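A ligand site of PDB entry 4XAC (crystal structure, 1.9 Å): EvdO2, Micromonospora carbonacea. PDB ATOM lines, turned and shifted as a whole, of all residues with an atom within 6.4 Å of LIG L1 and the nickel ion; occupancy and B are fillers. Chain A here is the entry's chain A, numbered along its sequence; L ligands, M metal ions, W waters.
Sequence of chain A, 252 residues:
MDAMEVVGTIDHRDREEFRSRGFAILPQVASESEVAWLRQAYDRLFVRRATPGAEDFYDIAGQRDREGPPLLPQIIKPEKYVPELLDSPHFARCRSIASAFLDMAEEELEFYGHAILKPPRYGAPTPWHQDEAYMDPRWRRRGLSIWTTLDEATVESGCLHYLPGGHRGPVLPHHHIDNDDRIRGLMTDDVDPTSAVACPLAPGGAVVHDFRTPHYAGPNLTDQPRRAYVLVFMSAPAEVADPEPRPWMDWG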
ATOM      1  N   LEU A  72     -26.359 -24.569 -21.949  1.00  0.00           N
ATOM      2  CA  LEU A  72     -27.720 -24.062 -21.975  1.00  0.00           C
ATOM      3  C   LEU A  72     -28.584 -24.970 -22.837  1.00  0.00           C
ATOM      4  O   LEU A  72     -28.255 -25.180 -24.007  1.00  0.00           O
ATOM      5  CB  LEU A  72     -27.722 -22.624 -22.508  1.00  0.00           C
ATOM      6  CG  LEU A  72     -29.047 -21.860 -22.555  1.00  0.00           C
ATOM      7  CD1 LEU A  72     -29.611 -21.724 -21.165  1.00  0.00           C
ATOM      8  CD2 LEU A  72     -28.815 -20.490 -23.176  1.00  0.00           C
ATOM      9  N   HIS A 114     -35.161 -21.036 -33.117  1.00  0.00           N
ATOM     10  CA  HIS A 114     -34.186 -21.481 -32.138  1.00  0.00           C
ATOM     11  C   HIS A 114     -34.893 -21.497 -30.786  1.00  0.00           C
ATOM     12  O   HIS A 114     -35.515 -20.511 -30.403  1.00  0.00           O
ATOM     13  CB  HIS A 114     -32.975 -20.551 -32.138  1.00  0.00           C
ATOM     14  CG  HIS A 114     -31.901 -20.936 -31.165  1.00  0.00           C
ATOM     15  ND1 HIS A 114     -31.110 -20.010 -30.529  1.00  0.00           N
ATOM     16  CD2 HIS A 114     -31.501 -22.144 -30.722  1.00  0.00           C
ATOM     17  CE1 HIS A 114     -30.255 -20.626 -29.740  1.00  0.00           C
ATOM     18  NE2 HIS A 114     -30.476 -21.933 -29.832  1.00  0.00           N
ATOM     19  N   ILE A 116     -34.860 -22.097 -26.589  1.00  0.00           N
ATOM     20  CA  ILE A 116     -34.012 -22.067 -25.413  1.00  0.00           C
ATOM     21  C   ILE A 116     -34.860 -22.327 -24.185  1.00  0.00           C
ATOM     22  O   ILE A 116     -36.020 -21.890 -24.087  1.00  0.00           O
ATOM     23  CB  ILE A 116     -33.286 -20.720 -25.267  1.00  0.00           C
ATOM     24  CG1 ILE A 116     -32.570 -20.343 -26.560  1.00  0.00           C
ATOM     25  CG2 ILE A 116     -32.293 -20.778 -24.121  1.00  0.00           C
ATOM     26  CD1 ILE A 116     -32.011 -18.948 -26.554  1.00  0.00           C
ATOM     27  N   LYS A 118     -34.001 -22.085 -20.050  1.00  0.00           N
ATOM     28  CA  LYS A 118     -33.181 -21.950 -18.844  1.00  0.00           C
ATOM     29  C   LYS A 118     -33.901 -22.672 -17.731  1.00  0.00           C
ATOM     30  O   LYS A 118     -34.940 -22.184 -17.263  1.00  0.00           O
ATOM     31  CB  LYS A 118     -32.948 -20.482 -18.463  1.00  0.00           C
ATOM     32  CG  LYS A 118     -31.925 -19.756 -19.338  1.00  0.00           C
ATOM     33  CD  LYS A 118     -31.450 -18.474 -18.651  1.00  0.00           C
ATOM     34  CE  LYS A 118     -29.934 -18.478 -18.396  1.00  0.00           C
ATOM     35  NZ  LYS A 118     -29.106 -18.035 -19.559  1.00  0.00           N
ATOM     36  N   PRO A 125     -24.727 -17.559 -16.783  1.00  0.00           N
ATOM     37  CA  PRO A 125     -25.351 -16.530 -17.623  1.00  0.00           C
ATOM     38  C   PRO A 125     -25.166 -16.878 -19.078  1.00  0.00           C
ATOM     39  O   PRO A 125     -24.427 -17.821 -19.385  1.00  0.00           O
ATOM     40  CB  PRO A 125     -24.574 -15.255 -17.263  1.00  0.00           C
ATOM     41  CG  PRO A 125     -23.168 -15.796 -16.939  1.00  0.00           C
ATOM     42  CD  PRO A 125     -23.368 -17.174 -16.341  1.00  0.00           C
ATOM     43  N   THR A 126     -25.832 -16.163 -19.971  1.00  0.00           N
ATOM     44  CA  THR A 126     -25.414 -16.137 -21.358  1.00  0.00           C
ATOM     45  C   THR A 126     -24.526 -14.903 -21.454  1.00  0.00           C
ATOM     46  O   THR A 126     -25.014 -13.782 -21.365  1.00  0.00           O
ATOM     47  CB  THR A 126     -26.604 -16.010 -22.348  1.00  0.00           C
ATOM     48  OG1 THR A 126     -27.531 -17.081 -22.121  1.00  0.00           O
ATOM     49  CG2 THR A 126     -26.099 -16.067 -23.778  1.00  0.00           C
ATOM     50  N   HIS A 129     -22.323 -10.987 -25.834  1.00  0.00           N
ATOM     51  CA  HIS A 129     -21.945 -11.375 -27.185  1.00  0.00           C
ATOM     52  C   HIS A 129     -22.758 -10.579 -28.203  1.00  0.00           C
ATOM     53  O   HIS A 129     -23.778  -9.972 -27.852  1.00  0.00           O
ATOM     54  CB  HIS A 129     -22.152 -12.896 -27.391  1.00  0.00           C
ATOM     55  CG  HIS A 129     -23.601 -13.295 -27.467  1.00  0.00           C
ATOM     56  ND1 HIS A 129     -24.393 -13.401 -26.337  1.00  0.00           N
ATOM     57  CD2 HIS A 129     -24.405 -13.562 -28.520  1.00  0.00           C
ATOM     58  CE1 HIS A 129     -25.627 -13.725 -26.698  1.00  0.00           C
ATOM     59  NE2 HIS A 129     -25.662 -13.822 -28.021  1.00  0.00           N
ATOM     60  N   GLN A 130     -22.292 -10.586 -29.444  1.00  0.00           N
ATOM     61  CA  GLN A 130     -23.081 -10.131 -30.569  1.00  0.00           C
ATOM     62  C   GLN A 130     -23.356 -11.327 -31.463  1.00  0.00           C
ATOM     63  O   GLN A 130     -22.479 -12.154 -31.708  1.00  0.00           O
ATOM     64  CB  GLN A 130     -22.343  -9.037 -31.355  1.00  0.00           C
ATOM     65  CG  GLN A 130     -22.209  -7.736 -30.604  1.00  0.00           C
ATOM     66  CD  GLN A 130     -21.039  -6.943 -31.129  1.00  0.00           C
ATOM     67  OE1 GLN A 130     -19.889  -7.381 -31.017  1.00  0.00           O
ATOM     68  NE2 GLN A 130     -21.329  -5.817 -31.755  1.00  0.00           N
ATOM     69  N   ASP A 131     -24.579 -11.449 -31.947  1.00  0.00           N
ATOM     70  CA  ASP A 131     -24.942 -12.624 -32.726  1.00  0.00           C
ATOM     71  C   ASP A 131     -24.108 -12.687 -34.016  1.00  0.00           C
ATOM     72  O   ASP A 131     -23.781 -13.767 -34.509  1.00  0.00           O
ATOM     73  CB  ASP A 131     -26.449 -12.613 -33.022  1.00  0.00           C
ATOM     74  CG  ASP A 131     -27.283 -12.778 -31.755  1.00  0.00           C
ATOM     75  OD1 ASP A 131     -26.762 -13.312 -30.760  1.00  0.00           O
ATOM     76  OD2 ASP A 131     -28.464 -12.367 -31.746  1.00  0.00           O
ATOM     77  N   TYR A 134     -20.902 -14.874 -34.537  1.00  0.00           N
ATOM     78  CA  TYR A 134     -20.990 -16.283 -34.913  1.00  0.00           C
ATOM     79  C   TYR A 134     -21.029 -16.469 -36.418  1.00  0.00           C
ATOM     80  O   TYR A 134     -21.036 -17.593 -36.919  1.00  0.00           O
ATOM     81  CB  TYR A 134     -22.239 -16.928 -34.305  1.00  0.00           C
ATOM     82  CG  TYR A 134     -22.168 -17.194 -32.826  1.00  0.00           C
ATOM     83  CD1 TYR A 134     -21.606 -18.373 -32.328  1.00  0.00           C
ATOM     84  CD2 TYR A 134     -22.701 -16.285 -31.899  1.00  0.00           C
ATOM     85  CE1 TYR A 134     -21.548 -18.632 -30.953  1.00  0.00           C
ATOM     86  CE2 TYR A 134     -22.642 -16.543 -30.524  1.00  0.00           C
ATOM     87  CZ  TYR A 134     -22.071 -17.717 -30.067  1.00  0.00           C
ATOM     88  OH  TYR A 134     -22.017 -17.972 -28.700  1.00  0.00           O
ATOM     89  N   SER A 145     -33.188 -10.769 -34.533  1.00  0.00           N
ATOM     90  CA  SER A 145     -33.756 -11.897 -33.816  1.00  0.00           C
ATOM     91  C   SER A 145     -34.962 -11.422 -33.036  1.00  0.00           C
ATOM     92  O   SER A 145     -34.913 -10.360 -32.439  1.00  0.00           O
ATOM     93  CB  SER A 145     -32.726 -12.523 -32.872  1.00  0.00           C
ATOM     94  OG  SER A 145     -31.635 -13.033 -33.625  1.00  0.00           O
ATOM     95  N   TRP A 147     -37.050 -12.583 -29.894  1.00  0.00           N
ATOM     96  CA  TRP A 147     -36.970 -13.467 -28.740  1.00  0.00           C
ATOM     97  C   TRP A 147     -38.299 -13.408 -28.001  1.00  0.00           C
ATOM     98  O   TRP A 147     -38.547 -12.463 -27.268  1.00  0.00           O
ATOM     99  CB  TRP A 147     -35.798 -12.993 -27.860  1.00  0.00           C
ATOM    100  CG  TRP A 147     -35.284 -13.821 -26.688  1.00  0.00           C
ATOM    101  CD1 TRP A 147     -34.205 -14.690 -26.696  1.00  0.00           C
ATOM    102  CD2 TRP A 147     -35.712 -13.738 -25.318  1.00  0.00           C
ATOM    103  NE1 TRP A 147     -33.986 -15.182 -25.420  1.00  0.00           N
ATOM    104  CE2 TRP A 147     -34.885 -14.612 -24.564  1.00  0.00           C
ATOM    105  CE3 TRP A 147     -36.716 -13.021 -24.656  1.00  0.00           C
ATOM    106  CZ2 TRP A 147     -35.042 -14.791 -23.183  1.00  0.00           C
ATOM    107  CZ3 TRP A 147     -36.869 -13.205 -23.267  1.00  0.00           C
ATOM    108  CH2 TRP A 147     -36.045 -14.087 -22.566  1.00  0.00           C
ATOM    109  N   GLY A 158     -33.562 -14.513 -15.925  1.00  0.00           N
ATOM    110  CA  GLY A 158     -32.751 -14.563 -17.131  1.00  0.00           C
ATOM    111  C   GLY A 158     -33.233 -13.784 -18.347  1.00  0.00           C
ATOM    112  O   GLY A 158     -33.050 -14.242 -19.473  1.00  0.00           O
ATOM    113  N   LEU A 160     -33.148 -10.672 -21.145  1.00  0.00           N
ATOM    114  CA  LEU A 160     -32.023 -10.120 -21.889  1.00  0.00           C
ATOM    115  C   LEU A 160     -31.662  -8.717 -21.416  1.00  0.00           C
ATOM    116  O   LEU A 160     -32.523  -7.955 -20.971  1.00  0.00           O
ATOM    117  CB  LEU A 160     -32.329 -10.103 -23.397  1.00  0.00           C
ATOM    118  CG  LEU A 160     -32.573 -11.502 -24.005  1.00  0.00           C
ATOM    119  CD1 LEU A 160     -32.508 -11.492 -25.540  1.00  0.00           C
ATOM    120  CD2 LEU A 160     -31.572 -12.514 -23.450  1.00  0.00           C
ATOM    121  N   HIS A 209     -33.717  -7.802 -31.484  1.00  0.00           N
ATOM    122  CA  HIS A 209     -32.427  -7.128 -31.582  1.00  0.00           C
ATOM    123  C   HIS A 209     -31.678  -7.409 -32.878  1.00  0.00           C
ATOM    124  O   HIS A 209     -31.743  -8.508 -33.432  1.00  0.00           O
ATOM    125  CB  HIS A 209     -31.512  -7.467 -30.375  1.00  0.00           C
ATOM    126  CG  HIS A 209     -31.224  -8.923 -30.190  1.00  0.00           C
ATOM    127  ND1 HIS A 209     -31.940  -9.722 -29.321  1.00  0.00           N
ATOM    128  CD2 HIS A 209     -30.248  -9.717 -30.708  1.00  0.00           C
ATOM    129  CE1 HIS A 209     -31.456 -10.946 -29.345  1.00  0.00           C
ATOM    130  NE2 HIS A 209     -30.429 -10.976 -30.177  1.00  0.00           N
ATOM    131  N   HIS A 215     -25.639  -8.276 -26.348  1.00  0.00           N
ATOM    132  CA  HIS A 215     -26.601  -8.685 -25.328  1.00  0.00           C
ATOM    133  C   HIS A 215     -26.076  -9.787 -24.425  1.00  0.00           C
ATOM    134  O   HIS A 215     -25.098 -10.487 -24.732  1.00  0.00           O
ATOM    135  CB  HIS A 215     -27.932  -9.100 -25.979  1.00  0.00           C
ATOM    136  CG  HIS A 215     -27.799 -10.153 -27.039  1.00  0.00           C
ATOM    137  ND1 HIS A 215     -27.348  -9.879 -28.311  1.00  0.00           N
ATOM    138  CD2 HIS A 215     -28.099 -11.474 -27.026  1.00  0.00           C
ATOM    139  CE1 HIS A 215     -27.353 -10.989 -29.022  1.00  0.00           C
ATOM    140  NE2 HIS A 215     -27.795 -11.967 -28.269  1.00  0.00           N
ATOM    141  N   TYR A 216     -26.756  -9.921 -23.288  1.00  0.00           N
ATOM    142  CA  TYR A 216     -26.352 -10.766 -22.172  1.00  0.00           C
ATOM    143  C   TYR A 216     -27.620 -11.282 -21.514  1.00  0.00           C
ATOM    144  O   TYR A 216     -28.643 -10.568 -21.515  1.00  0.00           O
ATOM    145  CB  TYR A 216     -25.512  -9.953 -21.189  1.00  0.00           C
ATOM    146  CG  TYR A 216     -25.401 -10.517 -19.794  1.00  0.00           C
ATOM    147  CD1 TYR A 216     -26.354 -10.207 -18.818  1.00  0.00           C
ATOM    148  CD2 TYR A 216     -24.330 -11.311 -19.442  1.00  0.00           C
ATOM    149  CE1 TYR A 216     -26.241 -10.703 -17.530  1.00  0.00           C
ATOM    150  CE2 TYR A 216     -24.216 -11.819 -18.148  1.00  0.00           C
ATOM    151  CZ  TYR A 216     -25.175 -11.500 -17.201  1.00  0.00           C
ATOM    152  OH  TYR A 216     -25.083 -11.995 -15.925  1.00  0.00           O
ATOM    153  N   ALA A 217     -27.585 -12.493 -20.964  1.00  0.00           N
ATOM    154  CA  ALA A 217     -28.701 -12.966 -20.148  1.00  0.00           C
ATOM    155  C   ALA A 217     -28.186 -13.477 -18.808  1.00  0.00           C
ATOM    156  O   ALA A 217     -27.242 -14.259 -18.753  1.00  0.00           O
ATOM    157  CB  ALA A 217     -29.498 -14.057 -20.875  1.00  0.00           C
ATOM    158  N   GLY A 218     -28.810 -13.033 -17.724  1.00  0.00           N
ATOM    159  CA  GLY A 218     -28.411 -13.478 -16.408  1.00  0.00           C
ATOM    160  C   GLY A 218     -28.806 -14.918 -16.141  1.00  0.00           C
ATOM    161  O   GLY A 218     -29.504 -15.532 -16.947  1.00  0.00           O
ATOM    162  N   ALA A 228     -37.776 -19.569 -24.017  1.00  0.00           N
ATOM    163  CA  ALA A 228     -37.843 -18.551 -25.062  1.00  0.00           C
ATOM    164  C   ALA A 228     -37.829 -19.229 -26.411  1.00  0.00           C
ATOM    165  O   ALA A 228     -37.203 -20.287 -26.591  1.00  0.00           O
ATOM    166  CB  ALA A 228     -36.686 -17.565 -24.963  1.00  0.00           C
ATOM    167  N   VAL A 230     -37.032 -18.237 -30.285  1.00  0.00           N
ATOM    168  CA  VAL A 230     -36.398 -17.171 -31.048  1.00  0.00           C
ATOM    169  C   VAL A 230     -36.606 -17.390 -32.530  1.00  0.00           C
ATOM    170  O   VAL A 230     -36.425 -18.497 -33.022  1.00  0.00           O
ATOM    171  CB  VAL A 230     -34.892 -17.081 -30.752  1.00  0.00           C
ATOM    172  CG1 VAL A 230     -34.304 -15.814 -31.388  1.00  0.00           C
ATOM    173  CG2 VAL A 230     -34.648 -17.062 -29.239  1.00  0.00           C
HETATM  174  C1  LIG L   1     -30.202 -14.502 -28.690  1.00  0.00           C
HETATM  175  O1  LIG L   1     -31.441 -14.662 -28.839  1.00  0.00           O
HETATM  176  O2  LIG L   1     -29.477 -14.060 -29.613  1.00  0.00           O
HETATM  177  C2  LIG L   1     -29.562 -14.858 -27.387  1.00  0.00           C
HETATM  178  O3  LIG L   1     -28.340 -14.795 -27.263  1.00  0.00           O
HETATM  179  C3  LIG L   1     -30.411 -15.328 -26.262  1.00  0.00           C
HETATM  180  C4  LIG L   1     -29.752 -15.678 -24.968  1.00  0.00           C
HETATM  181  C5  LIG L   1     -30.590 -16.316 -23.908  1.00  0.00           C
HETATM  182  O4  LIG L   1     -31.810 -16.538 -24.112  1.00  0.00           O
HETATM  183  O5  LIG L   1     -30.087 -16.625 -22.791  1.00  0.00           O
HETATM  184  N1  LG2 L   2     -26.405 -17.495 -30.732  1.00  0.00           N
HETATM  185  C1  LG2 L   2     -26.577 -16.145 -30.723  1.00  0.00           C
HETATM  186  N2  LG2 L   2     -27.272 -15.797 -29.618  1.00  0.00           N
HETATM  187  C2  LG2 L   2     -27.544 -16.923 -28.928  1.00  0.00           C
HETATM  188  C3  LG2 L   2     -26.997 -17.992 -29.625  1.00  0.00           C
HETATM  189 NI    NI M   1     -27.526 -13.922 -28.955  1.00  0.00          NI
HETATM  190  O   HOH W   1     -30.334 -15.045 -32.197  1.00  0.00           O
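A ring nitrogen (NE2) of His 209 lies close to an oxygen (O2) of LIG L1. NE1 of Trp 147 lies within hydrogen-bond range of O4 of LIG L1 (2.9 Å). An oxygen (O5) of LIG L1 lies within salt-bridge range of the side-chain amino group (NZ) of Lys 118, at 3.7 Å. An oxygen (O5) of LIG L1 sits at hydrogen-bond distance from the side-chain hydroxyl of Thr 126.
A ring nitrogen (NE2) of His 215 sits close to a ring nitrogen (NE2) of His 209 (3.4 Å). The side-chain hydroxyl (OG1) of Thr 126 sits at hydrogen-bond distance from the side-chain amino group (NZ) of Lys 118 (3.2 Å). N of Ser 145 is in hydrogen-bond range of O of His 209 (2.9 Å). The backbone carbonyl oxygen (O) of Ile 116 is in hydrogen-bond range of the backbone NH (N) of Ala 228 (2.9 Å). The backbone carbonyl oxygen (O) of Ala 217 sits at hydrogen-bond distance from the backbone NH (N) of Thr 126 (2.7 Å). A ring nitrogen (NE2) of His 209 sits at hydrogen-bond distance from the side-chain carboxylate of Asp 131 (2.9 Å).
Residues that only touch LIG L1: Ile 116, Leu 160 and Ala 217. Ten residues have an atom within 4 Å of LIG L1: Ile 116, Lys 118, Thr 126, His 129, Asp 131, Trp 147, Leu 160, His 209, His 215 and Ala 217. Along chain A the residues within 4 Å of LIG L1 span positions 116 to 217.
The nearest printed residue that does not touch the nickel ion is His 209 (4.3 Å).
The nickel ion is bound by a nitrogen (N2) of LG2 L2 (2.0 Å), the side-chain carboxylate (OD1) of Asp 131 (2.1 Å), an oxygen (O2) of LIG L1 (2.1 Å), an oxygen (O3) of LIG L1 (2.1 Å), a ring nitrogen (NE2) of His 129 (2.1 Å) and a ring nitrogen (NE2) of His 215 (2.1 Å). The nickel ion has six donor atoms within binding distance.
Water W1 lies within hydrogen-bond range of the side-chain hydroxyl (OG) of Ser 145 (2.8 Å) and the side-chain carboxylate (OD2) of Asp 131 (3.3 Å).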
